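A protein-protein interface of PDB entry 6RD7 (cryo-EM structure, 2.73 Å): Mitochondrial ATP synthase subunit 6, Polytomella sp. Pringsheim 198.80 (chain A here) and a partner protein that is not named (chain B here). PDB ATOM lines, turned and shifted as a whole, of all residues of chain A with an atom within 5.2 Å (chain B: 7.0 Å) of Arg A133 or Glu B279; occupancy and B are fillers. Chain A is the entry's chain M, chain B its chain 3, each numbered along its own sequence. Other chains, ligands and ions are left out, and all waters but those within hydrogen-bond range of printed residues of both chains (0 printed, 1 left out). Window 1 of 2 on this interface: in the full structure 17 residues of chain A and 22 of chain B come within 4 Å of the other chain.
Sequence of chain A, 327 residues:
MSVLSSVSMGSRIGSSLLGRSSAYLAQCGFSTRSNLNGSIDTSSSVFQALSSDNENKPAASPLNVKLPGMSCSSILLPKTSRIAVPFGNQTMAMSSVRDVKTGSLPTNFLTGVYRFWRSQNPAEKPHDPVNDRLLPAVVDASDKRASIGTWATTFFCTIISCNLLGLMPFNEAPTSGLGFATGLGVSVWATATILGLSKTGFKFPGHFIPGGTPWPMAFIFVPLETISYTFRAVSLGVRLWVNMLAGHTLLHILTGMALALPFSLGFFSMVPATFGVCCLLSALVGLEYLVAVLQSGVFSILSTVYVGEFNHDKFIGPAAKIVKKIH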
ATOM      1  N   ASN A 131      17.753 -26.677 -11.951  1.00  0.00           N
ATOM      2  CA  ASN A 131      17.534 -25.334 -11.435  1.00  0.00           C
ATOM      3  C   ASN A 131      16.809 -25.481 -10.104  1.00  0.00           C
ATOM      4  O   ASN A 131      16.783 -26.569  -9.519  1.00  0.00           O
ATOM      5  CB  ASN A 131      16.766 -24.464 -12.435  1.00  0.00           C
ATOM      6  CG  ASN A 131      15.654 -25.211 -13.137  1.00  0.00           C
ATOM      7  OD1 ASN A 131      14.932 -25.996 -12.531  1.00  0.00           O
ATOM      8  ND2 ASN A 131      15.506 -24.959 -14.428  1.00  0.00           N
ATOM      9  N   ASP A 132      16.209 -24.387  -9.626  1.00  0.00           N
ATOM     10  CA  ASP A 132      15.553 -24.401  -8.319  1.00  0.00           C
ATOM     11  C   ASP A 132      14.308 -25.278  -8.316  1.00  0.00           C
ATOM     12  O   ASP A 132      13.846 -25.704  -7.253  1.00  0.00           O
ATOM     13  CB  ASP A 132      15.196 -22.978  -7.898  1.00  0.00           C
ATOM     14  CG  ASP A 132      16.390 -22.203  -7.400  1.00  0.00           C
ATOM     15  OD1 ASP A 132      17.529 -22.659  -7.626  1.00  0.00           O
ATOM     16  OD2 ASP A 132      16.194 -21.141  -6.775  1.00  0.00           O
ATOM     17  N   ARG A 133      13.744 -25.550  -9.492  1.00  0.00           N
ATOM     18  CA  ARG A 133      12.644 -26.501  -9.579  1.00  0.00           C
ATOM     19  C   ARG A 133      13.133 -27.926  -9.350  1.00  0.00           C
ATOM     20  O   ARG A 133      12.481 -28.711  -8.653  1.00  0.00           O
ATOM     21  CB  ARG A 133      11.958 -26.373 -10.938  1.00  0.00           C
ATOM     22  CG  ARG A 133      10.812 -27.330 -11.150  1.00  0.00           C
ATOM     23  CD  ARG A 133       9.679 -27.024 -10.204  1.00  0.00           C
ATOM     24  NE  ARG A 133       8.475 -27.768 -10.543  1.00  0.00           N
ATOM     25  CZ  ARG A 133       8.071 -28.856  -9.902  1.00  0.00           C
ATOM     26  NH1 ARG A 133       8.778 -29.328  -8.890  1.00  0.00           N
ATOM     27  NH2 ARG A 133       6.961 -29.474 -10.274  1.00  0.00           N
ATOM     28  N   LEU A 134      14.287 -28.271  -9.913  1.00  0.00           N
ATOM     29  CA  LEU A 134      14.834 -29.618  -9.826  1.00  0.00           C
ATOM     30  C   LEU A 134      15.764 -29.816  -8.636  1.00  0.00           C
ATOM     31  O   LEU A 134      16.173 -30.950  -8.377  1.00  0.00           O
ATOM     32  CB  LEU A 134      15.585 -29.959 -11.114  1.00  0.00           C
ATOM     33  CG  LEU A 134      15.561 -31.420 -11.550  1.00  0.00           C
ATOM     34  CD1 LEU A 134      14.174 -31.807 -12.007  1.00  0.00           C
ATOM     35  CD2 LEU A 134      16.590 -31.669 -12.628  1.00  0.00           C
ATOM     36  N   LEU A 135      16.111 -28.746  -7.924  1.00  0.00           N
ATOM     37  CA  LEU A 135      17.022 -28.855  -6.783  1.00  0.00           C
ATOM     38  C   LEU A 135      16.524 -29.738  -5.638  1.00  0.00           C
ATOM     39  O   LEU A 135      17.352 -30.478  -5.078  1.00  0.00           O
ATOM     40  CB  LEU A 135      17.379 -27.453  -6.279  1.00  0.00           C
ATOM     41  CG  LEU A 135      18.664 -26.839  -6.816  1.00  0.00           C
ATOM     42  CD1 LEU A 135      18.874 -25.497  -6.165  1.00  0.00           C
ATOM     43  CD2 LEU A 135      19.846 -27.752  -6.577  1.00  0.00           C
ATOM     44  N   PRO A 136      15.240 -29.724  -5.220  1.00  0.00           N
ATOM     45  CA  PRO A 136      14.857 -30.689  -4.176  1.00  0.00           C
ATOM     46  C   PRO A 136      14.848 -32.128  -4.643  1.00  0.00           C
ATOM     47  O   PRO A 136      15.097 -33.025  -3.836  1.00  0.00           O
ATOM     48  CB  PRO A 136      13.458 -30.223  -3.765  1.00  0.00           C
ATOM     49  CG  PRO A 136      13.394 -28.845  -4.149  1.00  0.00           C
ATOM     50  CD  PRO A 136      14.141 -28.757  -5.414  1.00  0.00           C
ATOM     51  N   ALA A 137      14.611 -32.374  -5.931  1.00  0.00           N
ATOM     52  CA  ALA A 137      14.713 -33.733  -6.443  1.00  0.00           C
ATOM     53  C   ALA A 137      16.163 -34.198  -6.483  1.00  0.00           C
ATOM     54  O   ALA A 137      16.447 -35.373  -6.238  1.00  0.00           O
ATOM     55  CB  ALA A 137      14.076 -33.819  -7.826  1.00  0.00           C
ATOM     56  N   PRO A 318       9.731 -33.479 -11.502  1.00  0.00           N
ATOM     57  CA  PRO A 318       8.480 -32.715 -11.483  1.00  0.00           C
ATOM     58  C   PRO A 318       7.304 -33.500 -12.040  1.00  0.00           C
ATOM     59  O   PRO A 318       7.377 -34.060 -13.138  1.00  0.00           O
ATOM     60  CB  PRO A 318       8.802 -31.493 -12.347  1.00  0.00           C
ATOM     61  CG  PRO A 318       9.893 -31.932 -13.244  1.00  0.00           C
ATOM     62  CD  PRO A 318      10.659 -33.009 -12.544  1.00  0.00           C
ATOM     63  N   ALA A 319       6.216 -33.555 -11.278  1.00  0.00           N
ATOM     64  CA  ALA A 319       4.980 -34.181 -11.721  1.00  0.00           C
ATOM     65  C   ALA A 319       4.057 -33.207 -12.433  1.00  0.00           C
ATOM     66  O   ALA A 319       2.979 -33.609 -12.880  1.00  0.00           O
ATOM     67  CB  ALA A 319       4.249 -34.807 -10.531  1.00  0.00           C
ATOM     68  N   ALA A 320       4.454 -31.943 -12.540  1.00  0.00           N
ATOM     69  CA  ALA A 320       3.659 -30.924 -13.216  1.00  0.00           C
ATOM     70  C   ALA A 320       4.603 -29.817 -13.640  1.00  0.00           C
ATOM     71  O   ALA A 320       5.428 -29.374 -12.836  1.00  0.00           O
ATOM     72  CB  ALA A 320       2.569 -30.382 -12.302  1.00  0.00           C
ATOM     73  N   LYS A 321       4.498 -29.375 -14.884  1.00  0.00           N
ATOM     74  CA  LYS A 321       5.344 -28.310 -15.393  1.00  0.00           C
ATOM     75  C   LYS A 321       4.482 -27.262 -16.072  1.00  0.00           C
ATOM     76  O   LYS A 321       3.290 -27.470 -16.307  1.00  0.00           O
ATOM     77  CB  LYS A 321       6.391 -28.832 -16.384  1.00  0.00           C
ATOM     78  CG  LYS A 321       7.545 -29.582 -15.742  1.00  0.00           C
ATOM     79  CD  LYS A 321       8.381 -28.695 -14.842  1.00  0.00           C
ATOM     80  CE  LYS A 321       9.306 -27.801 -15.646  1.00  0.00           C
ATOM     81  NZ  LYS A 321      10.603 -27.597 -14.952  1.00  0.00           N
ATOM     82  N   ILE A 322       5.094 -26.123 -16.366  1.00  0.00           N
ATOM     83  CA  ILE A 322       4.489 -25.089 -17.191  1.00  0.00           C
ATOM     84  C   ILE A 322       5.398 -24.954 -18.408  1.00  0.00           C
ATOM     85  O   ILE A 322       6.500 -24.404 -18.330  1.00  0.00           O
ATOM     86  CB  ILE A 322       4.307 -23.779 -16.419  1.00  0.00           C
ATOM     87  CG1 ILE A 322       3.178 -23.947 -15.399  1.00  0.00           C
ATOM     88  CG2 ILE A 322       3.988 -22.628 -17.347  1.00  0.00           C
ATOM     89  CD1 ILE A 322       2.747 -22.677 -14.706  1.00  0.00           C
ATOM     90  N   ARG B 242      11.650 -22.404  -2.969  1.00  0.00           N
ATOM     91  CA  ARG B 242      12.518 -23.513  -3.366  1.00  0.00           C
ATOM     92  C   ARG B 242      12.260 -24.783  -2.555  1.00  0.00           C
ATOM     93  O   ARG B 242      12.540 -25.886  -3.030  1.00  0.00           O
ATOM     94  CB  ARG B 242      13.980 -23.090  -3.232  1.00  0.00           C
ATOM     95  CG  ARG B 242      14.968 -23.965  -3.969  1.00  0.00           C
ATOM     96  CD  ARG B 242      16.338 -23.333  -4.040  1.00  0.00           C
ATOM     97  NE  ARG B 242      16.571 -22.374  -2.970  1.00  0.00           N
ATOM     98  CZ  ARG B 242      16.941 -21.116  -3.172  1.00  0.00           C
ATOM     99  NH1 ARG B 242      17.138 -20.309  -2.144  1.00  0.00           N
ATOM    100  NH2 ARG B 242      17.111 -20.664  -4.403  1.00  0.00           N
ATOM    101  N   PHE B 244       9.370 -26.042  -1.697  1.00  0.00           N
ATOM    102  CA  PHE B 244       8.157 -26.732  -2.116  1.00  0.00           C
ATOM    103  C   PHE B 244       8.449 -27.626  -3.310  1.00  0.00           C
ATOM    104  O   PHE B 244       9.036 -27.184  -4.301  1.00  0.00           O
ATOM    105  CB  PHE B 244       7.060 -25.729  -2.455  1.00  0.00           C
ATOM    106  CG  PHE B 244       6.414 -25.127  -1.250  1.00  0.00           C
ATOM    107  CD1 PHE B 244       5.573 -25.884  -0.453  1.00  0.00           C
ATOM    108  CD2 PHE B 244       6.659 -23.814  -0.902  1.00  0.00           C
ATOM    109  CE1 PHE B 244       4.982 -25.338   0.663  1.00  0.00           C
ATOM    110  CE2 PHE B 244       6.070 -23.264   0.212  1.00  0.00           C
ATOM    111  CZ  PHE B 244       5.230 -24.027   0.995  1.00  0.00           C
ATOM    112  N   SER B 245       8.033 -28.884  -3.219  1.00  0.00           N
ATOM    113  CA  SER B 245       8.465 -29.887  -4.179  1.00  0.00           C
ATOM    114  C   SER B 245       7.472 -31.034  -4.194  1.00  0.00           C
ATOM    115  O   SER B 245       6.550 -31.096  -3.382  1.00  0.00           O
ATOM    116  CB  SER B 245       9.855 -30.405  -3.837  1.00  0.00           C
ATOM    117  OG  SER B 245      10.250 -31.429  -4.727  1.00  0.00           O
ATOM    118  N   GLU B 246       7.680 -31.951  -5.138  1.00  0.00           N
ATOM    119  CA  GLU B 246       6.947 -33.208  -5.109  1.00  0.00           C
ATOM    120  C   GLU B 246       7.430 -34.084  -3.964  1.00  0.00           C
ATOM    121  O   GLU B 246       6.651 -34.853  -3.389  1.00  0.00           O
ATOM    122  CB  GLU B 246       7.098 -33.932  -6.444  1.00  0.00           C
ATOM    123  CG  GLU B 246       6.189 -33.406  -7.533  1.00  0.00           C
ATOM    124  CD  GLU B 246       6.796 -32.250  -8.301  1.00  0.00           C
ATOM    125  OE1 GLU B 246       7.932 -31.845  -7.980  1.00  0.00           O
ATOM    126  OE2 GLU B 246       6.133 -31.741  -9.227  1.00  0.00           O
ATOM    127  N   PRO B 275       6.847 -18.409  -8.655  1.00  0.00           N
ATOM    128  CA  PRO B 275       8.115 -19.007  -9.079  1.00  0.00           C
ATOM    129  C   PRO B 275       7.885 -20.237  -9.931  1.00  0.00           C
ATOM    130  O   PRO B 275       6.739 -20.556 -10.251  1.00  0.00           O
ATOM    131  CB  PRO B 275       8.774 -19.368  -7.750  1.00  0.00           C
ATOM    132  CG  PRO B 275       7.611 -19.738  -6.906  1.00  0.00           C
ATOM    133  CD  PRO B 275       6.494 -18.807  -7.284  1.00  0.00           C
ATOM    134  N   GLU B 276       8.952 -20.937 -10.309  1.00  0.00           N
ATOM    135  CA  GLU B 276       8.775 -22.200 -11.015  1.00  0.00           C
ATOM    136  C   GLU B 276       8.194 -23.263 -10.092  1.00  0.00           C
ATOM    137  O   GLU B 276       7.338 -24.058 -10.501  1.00  0.00           O
ATOM    138  CB  GLU B 276      10.108 -22.661 -11.598  1.00  0.00           C
ATOM    139  CG  GLU B 276       9.996 -23.289 -12.972  1.00  0.00           C
ATOM    140  CD  GLU B 276      11.327 -23.780 -13.506  1.00  0.00           C
ATOM    141  OE1 GLU B 276      11.324 -24.689 -14.361  1.00  0.00           O
ATOM    142  OE2 GLU B 276      12.374 -23.254 -13.074  1.00  0.00           O
ATOM    143  N   SER B 277       8.584 -23.238  -8.817  1.00  0.00           N
ATOM    144  CA  SER B 277       8.237 -24.309  -7.893  1.00  0.00           C
ATOM    145  C   SER B 277       6.767 -24.314  -7.506  1.00  0.00           C
ATOM    146  O   SER B 277       6.311 -25.273  -6.874  1.00  0.00           O
ATOM    147  CB  SER B 277       9.094 -24.207  -6.642  1.00  0.00           C
ATOM    148  OG  SER B 277      10.466 -24.350  -6.953  1.00  0.00           O
ATOM    149  N   ILE B 278       6.005 -23.288  -7.900  1.00  0.00           N
ATOM    150  CA  ILE B 278       4.563 -23.299  -7.704  1.00  0.00           C
ATOM    151  C   ILE B 278       3.904 -24.382  -8.554  1.00  0.00           C
ATOM    152  O   ILE B 278       2.805 -24.837  -8.215  1.00  0.00           O
ATOM    153  CB  ILE B 278       3.966 -21.897  -7.985  1.00  0.00           C
ATOM    154  CG1 ILE B 278       2.600 -21.740  -7.327  1.00  0.00           C
ATOM    155  CG2 ILE B 278       3.783 -21.647  -9.462  1.00  0.00           C
ATOM    156  CD1 ILE B 278       2.092 -20.330  -7.324  1.00  0.00           C
ATOM    157  N   GLU B 279       4.580 -24.852  -9.620  1.00  0.00           N
ATOM    158  CA  GLU B 279       4.110 -26.023 -10.359  1.00  0.00           C
ATOM    159  C   GLU B 279       4.029 -27.251  -9.464  1.00  0.00           C
ATOM    160  O   GLU B 279       3.177 -28.123  -9.669  1.00  0.00           O
ATOM    161  CB  GLU B 279       5.035 -26.319 -11.536  1.00  0.00           C
ATOM    162  CG  GLU B 279       5.165 -25.228 -12.565  1.00  0.00           C
ATOM    163  CD  GLU B 279       6.484 -25.313 -13.305  1.00  0.00           C
ATOM    164  OE1 GLU B 279       6.716 -24.498 -14.219  1.00  0.00           O
ATOM    165  OE2 GLU B 279       7.290 -26.202 -12.967  1.00  0.00           O
ATOM    166  N   ALA B 280       4.903 -27.337  -8.461  1.00  0.00           N
ATOM    167  CA  ALA B 280       4.839 -28.460  -7.539  1.00  0.00           C
ATOM    168  C   ALA B 280       3.679 -28.311  -6.568  1.00  0.00           C
ATOM    169  O   ALA B 280       3.171 -29.306  -6.043  1.00  0.00           O
ATOM    170  CB  ALA B 280       6.154 -28.592  -6.782  1.00  0.00           C
ATOM    171  N   VAL B 281       3.240 -27.077  -6.315  1.00  0.00           N
ATOM    172  CA  VAL B 281       2.168 -26.882  -5.346  1.00  0.00           C
ATOM    173  C   VAL B 281       0.813 -27.054  -6.017  1.00  0.00           C
ATOM    174  O   VAL B 281      -0.027 -27.836  -5.551  1.00  0.00           O
ATOM    175  CB  VAL B 281       2.295 -25.510  -4.664  1.00  0.00           C
ATOM    176  CG1 VAL B 281       1.398 -25.456  -3.446  1.00  0.00           C
ATOM    177  CG2 VAL B 281       3.733 -25.247  -4.276  1.00  0.00           C
ATOM    178  N   ILE B 282       0.598 -26.335  -7.128  1.00  0.00           N
ATOM    179  CA  ILE B 282      -0.635 -26.437  -7.910  1.00  0.00           C
ATOM    180  C   ILE B 282      -0.847 -27.865  -8.390  1.00  0.00           C
ATOM    181  O   ILE B 282      -1.959 -28.403  -8.302  1.00  0.00           O
ATOM    182  CB  ILE B 282      -0.597 -25.455  -9.096  1.00  0.00           C
ATOM    183  CG1 ILE B 282      -0.397 -24.022  -8.617  1.00  0.00           C
ATOM    184  CG2 ILE B 282      -1.867 -25.543  -9.911  1.00  0.00           C
ATOM    185  CD1 ILE B 282      -0.056 -23.069  -9.735  1.00  0.00           C
ATOM    186  N   GLY B 283       0.229 -28.509  -8.856  1.00  0.00           N
ATOM    187  CA  GLY B 283       0.153 -29.905  -9.251  1.00  0.00           C
ATOM    188  C   GLY B 283      -0.241 -30.821  -8.110  1.00  0.00           C
ATOM    189  O   GLY B 283      -1.012 -31.764  -8.303  1.00  0.00           O
ATOM    190  N   ALA B 284       0.201 -30.497  -6.889  1.00  0.00           N
ATOM    191  CA  ALA B 284      -0.166 -31.310  -5.733  1.00  0.00           C
ATOM    192  C   ALA B 284      -1.643 -31.159  -5.401  1.00  0.00           C
ATOM    193  O   ALA B 284      -2.219 -31.999  -4.702  1.00  0.00           O
ATOM    194  CB  ALA B 284       0.693 -30.936  -4.529  1.00  0.00           C
ATOM    195  N   ALA B 285      -2.272 -30.092  -5.895  1.00  0.00           N
ATOM    196  CA  ALA B 285      -3.719 -29.992  -5.794  1.00  0.00           C
ATOM    197  C   ALA B 285      -4.400 -30.740  -6.930  1.00  0.00           C
ATOM    198  O   ALA B 285      -5.455 -31.351  -6.731  1.00  0.00           O
ATOM    199  CB  ALA B 285      -4.145 -28.528  -5.783  1.00  0.00           C
ATOM    200  N   ALA B 307      -0.355 -17.983 -12.329  1.00  0.00           N
ATOM    201  CA  ALA B 307       0.996 -18.508 -12.497  1.00  0.00           C
ATOM    202  C   ALA B 307       1.286 -18.876 -13.944  1.00  0.00           C
ATOM    203  O   ALA B 307       2.447 -18.845 -14.365  1.00  0.00           O
ATOM    204  CB  ALA B 307       1.202 -19.720 -11.594  1.00  0.00           C
ATOM    205  N   LEU B 311       4.536 -17.029 -15.565  1.00  0.00           N
ATOM    206  CA  LEU B 311       5.630 -17.836 -16.086  1.00  0.00           C
ATOM    207  C   LEU B 311       5.603 -17.964 -17.601  1.00  0.00           C
ATOM    208  O   LEU B 311       6.547 -18.513 -18.177  1.00  0.00           O
ATOM    209  CB  LEU B 311       5.608 -19.224 -15.446  1.00  0.00           C
ATOM    210  CG  LEU B 311       5.990 -19.249 -13.968  1.00  0.00           C
ATOM    211  CD1 LEU B 311       5.437 -20.482 -13.298  1.00  0.00           C
ATOM    212  CD2 LEU B 311       7.494 -19.188 -13.814  1.00  0.00           C
ATOM    213  N   PHE B 315       0.038 -24.797 -17.908  1.00  0.00           N
ATOM    214  CA  PHE B 315       0.236 -25.800 -16.872  1.00  0.00           C
ATOM    215  C   PHE B 315      -0.157 -27.171 -17.407  1.00  0.00           C
ATOM    216  O   PHE B 315      -1.298 -27.369 -17.835  1.00  0.00           O
ATOM    217  CB  PHE B 315      -0.599 -25.431 -15.646  1.00  0.00           C
ATOM    218  CG  PHE B 315      -0.461 -26.377 -14.493  1.00  0.00           C
ATOM    219  CD1 PHE B 315       0.591 -26.251 -13.605  1.00  0.00           C
ATOM    220  CD2 PHE B 315      -1.408 -27.364 -14.272  1.00  0.00           C
ATOM    221  CE1 PHE B 315       0.711 -27.109 -12.535  1.00  0.00           C
ATOM    222  CE2 PHE B 315      -1.287 -28.225 -13.208  1.00  0.00           C
ATOM    223  CZ  PHE B 315      -0.232 -28.095 -12.338  1.00  0.00           C
ATOM    224  N   VAL B 316       0.776 -28.117 -17.366  1.00  0.00           N
ATOM    225  CA  VAL B 316       0.535 -29.484 -17.813  1.00  0.00           C
ATOM    226  C   VAL B 316       0.754 -30.421 -16.630  1.00  0.00           C
ATOM    227  O   VAL B 316       1.650 -30.199 -15.808  1.00  0.00           O
ATOM    228  CB  VAL B 316       1.422 -29.848 -19.027  1.00  0.00           C
ATOM    229  CG1 VAL B 316       2.919 -29.771 -18.713  1.00  0.00           C
ATOM    230  CG2 VAL B 316       1.057 -31.216 -19.594  1.00  0.00           C
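Printed residues of chain B that touch a printed residue of chain A: Arg B242, Ser B245, Glu B246, Glu B276, Ser B277, Glu B279, Ala B280, Gly B283, Ala B307, Leu B311, Phe B315 and Val B316.
Among the printed residues, 26 pairs touch across the chains.
Among the printed residues, Asp or Glu carboxylates within 4 Å of a Lys or Arg side-chain nitrogen of the other chain: Asp A132 with Arg B242 (2.6 Å), Arg A133 with Glu B246 (2.6 Å), Arg A133 with Glu B279 (3.1 Å) and Lys A321 with Glu B276 (3.1 Å).
OE2 of Glu B276 touches OD1 of Asn A131, at 3.8 Å.
OG of Ser B277 touches O of Asp A132 (3.7 Å).
Arg A133 touches Ser B277 (CD to CA, 3.8 Å).
Leu A135 touches Arg B242 (CD1 to CD, 3.95 Å).
Glu B279 touches Ala A320 (CB to O, 3.3 Å).
Ala A320 touches Val B316 (CA to O, 3.4 Å).
Lys A321 touches Glu B279.
O of Lys A321 touches CA of Phe B315 (3.5 Å).
Ile A322 touches Ala B307.
CA of Phe B315 touches CG1 of Ile A322 (3.8 Å).
O of Ala A320 is in hydrogen-bond range of NH2 of Arg A133, 3.0 Å away.
The side-chain amide oxygen (OD1) of Asn A131 sits close to the backbone NH (N) of Arg A133 (3.3 Å).
OE2 of Glu B246 lies within salt-bridge range of NH2 of Arg A133 (2.6 Å).
N of Val B316 is in hydrogen-bond range of O of Lys A321, at 2.8 Å.
NH2 of Arg B242 is in salt-bridge range of OD2 of Asp A132, 2.6 Å away.
The guanidinium group of Arg A133 sits close to the backbone NH of Ala B280 (3.5 Å).
The backbone NH of Ile A322 lies within hydrogen-bond range of the side-chain carboxylate of Glu B279, 3.1 Å away.
N of Ala A319 is in hydrogen-bond range of OE2 of Glu B246 (2.7 Å).
The side-chain carboxylate of Glu B279 is in salt-bridge range of the guanidinium group of Arg A133, at 3.1 Å.
NZ of Lys A321 is in salt-bridge range of OE1 of Glu B276 (3.1 Å).
Arg A133 touches just these residues of chain B: Glu B246, Glu B276, Ser B277, Glu B279 and Ala B280.
Printed residues of chain A within 4 Å of Glu B279: Arg A133, Ala A320, Lys A321 and Ile A322.
Printed residues of chain B within 4 Å of Asp A132: Arg B242 (2.6 Å) and Ser B277 (3.7 Å).
Of the printed residues of chain B, Pro A318 touches Glu B246.
Of the printed residues of chain A, Ser B245 touches Pro A136 (3.6 Å).
Phe B244 touches none of the printed residues of chain A.
The nearest printed residue of chain A that does not touch Glu B279 is Pro A318 (5.5 Å).
The nearest printed residue of chain A that does not touch Ala B307 is Lys A321 (8.8 Å).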
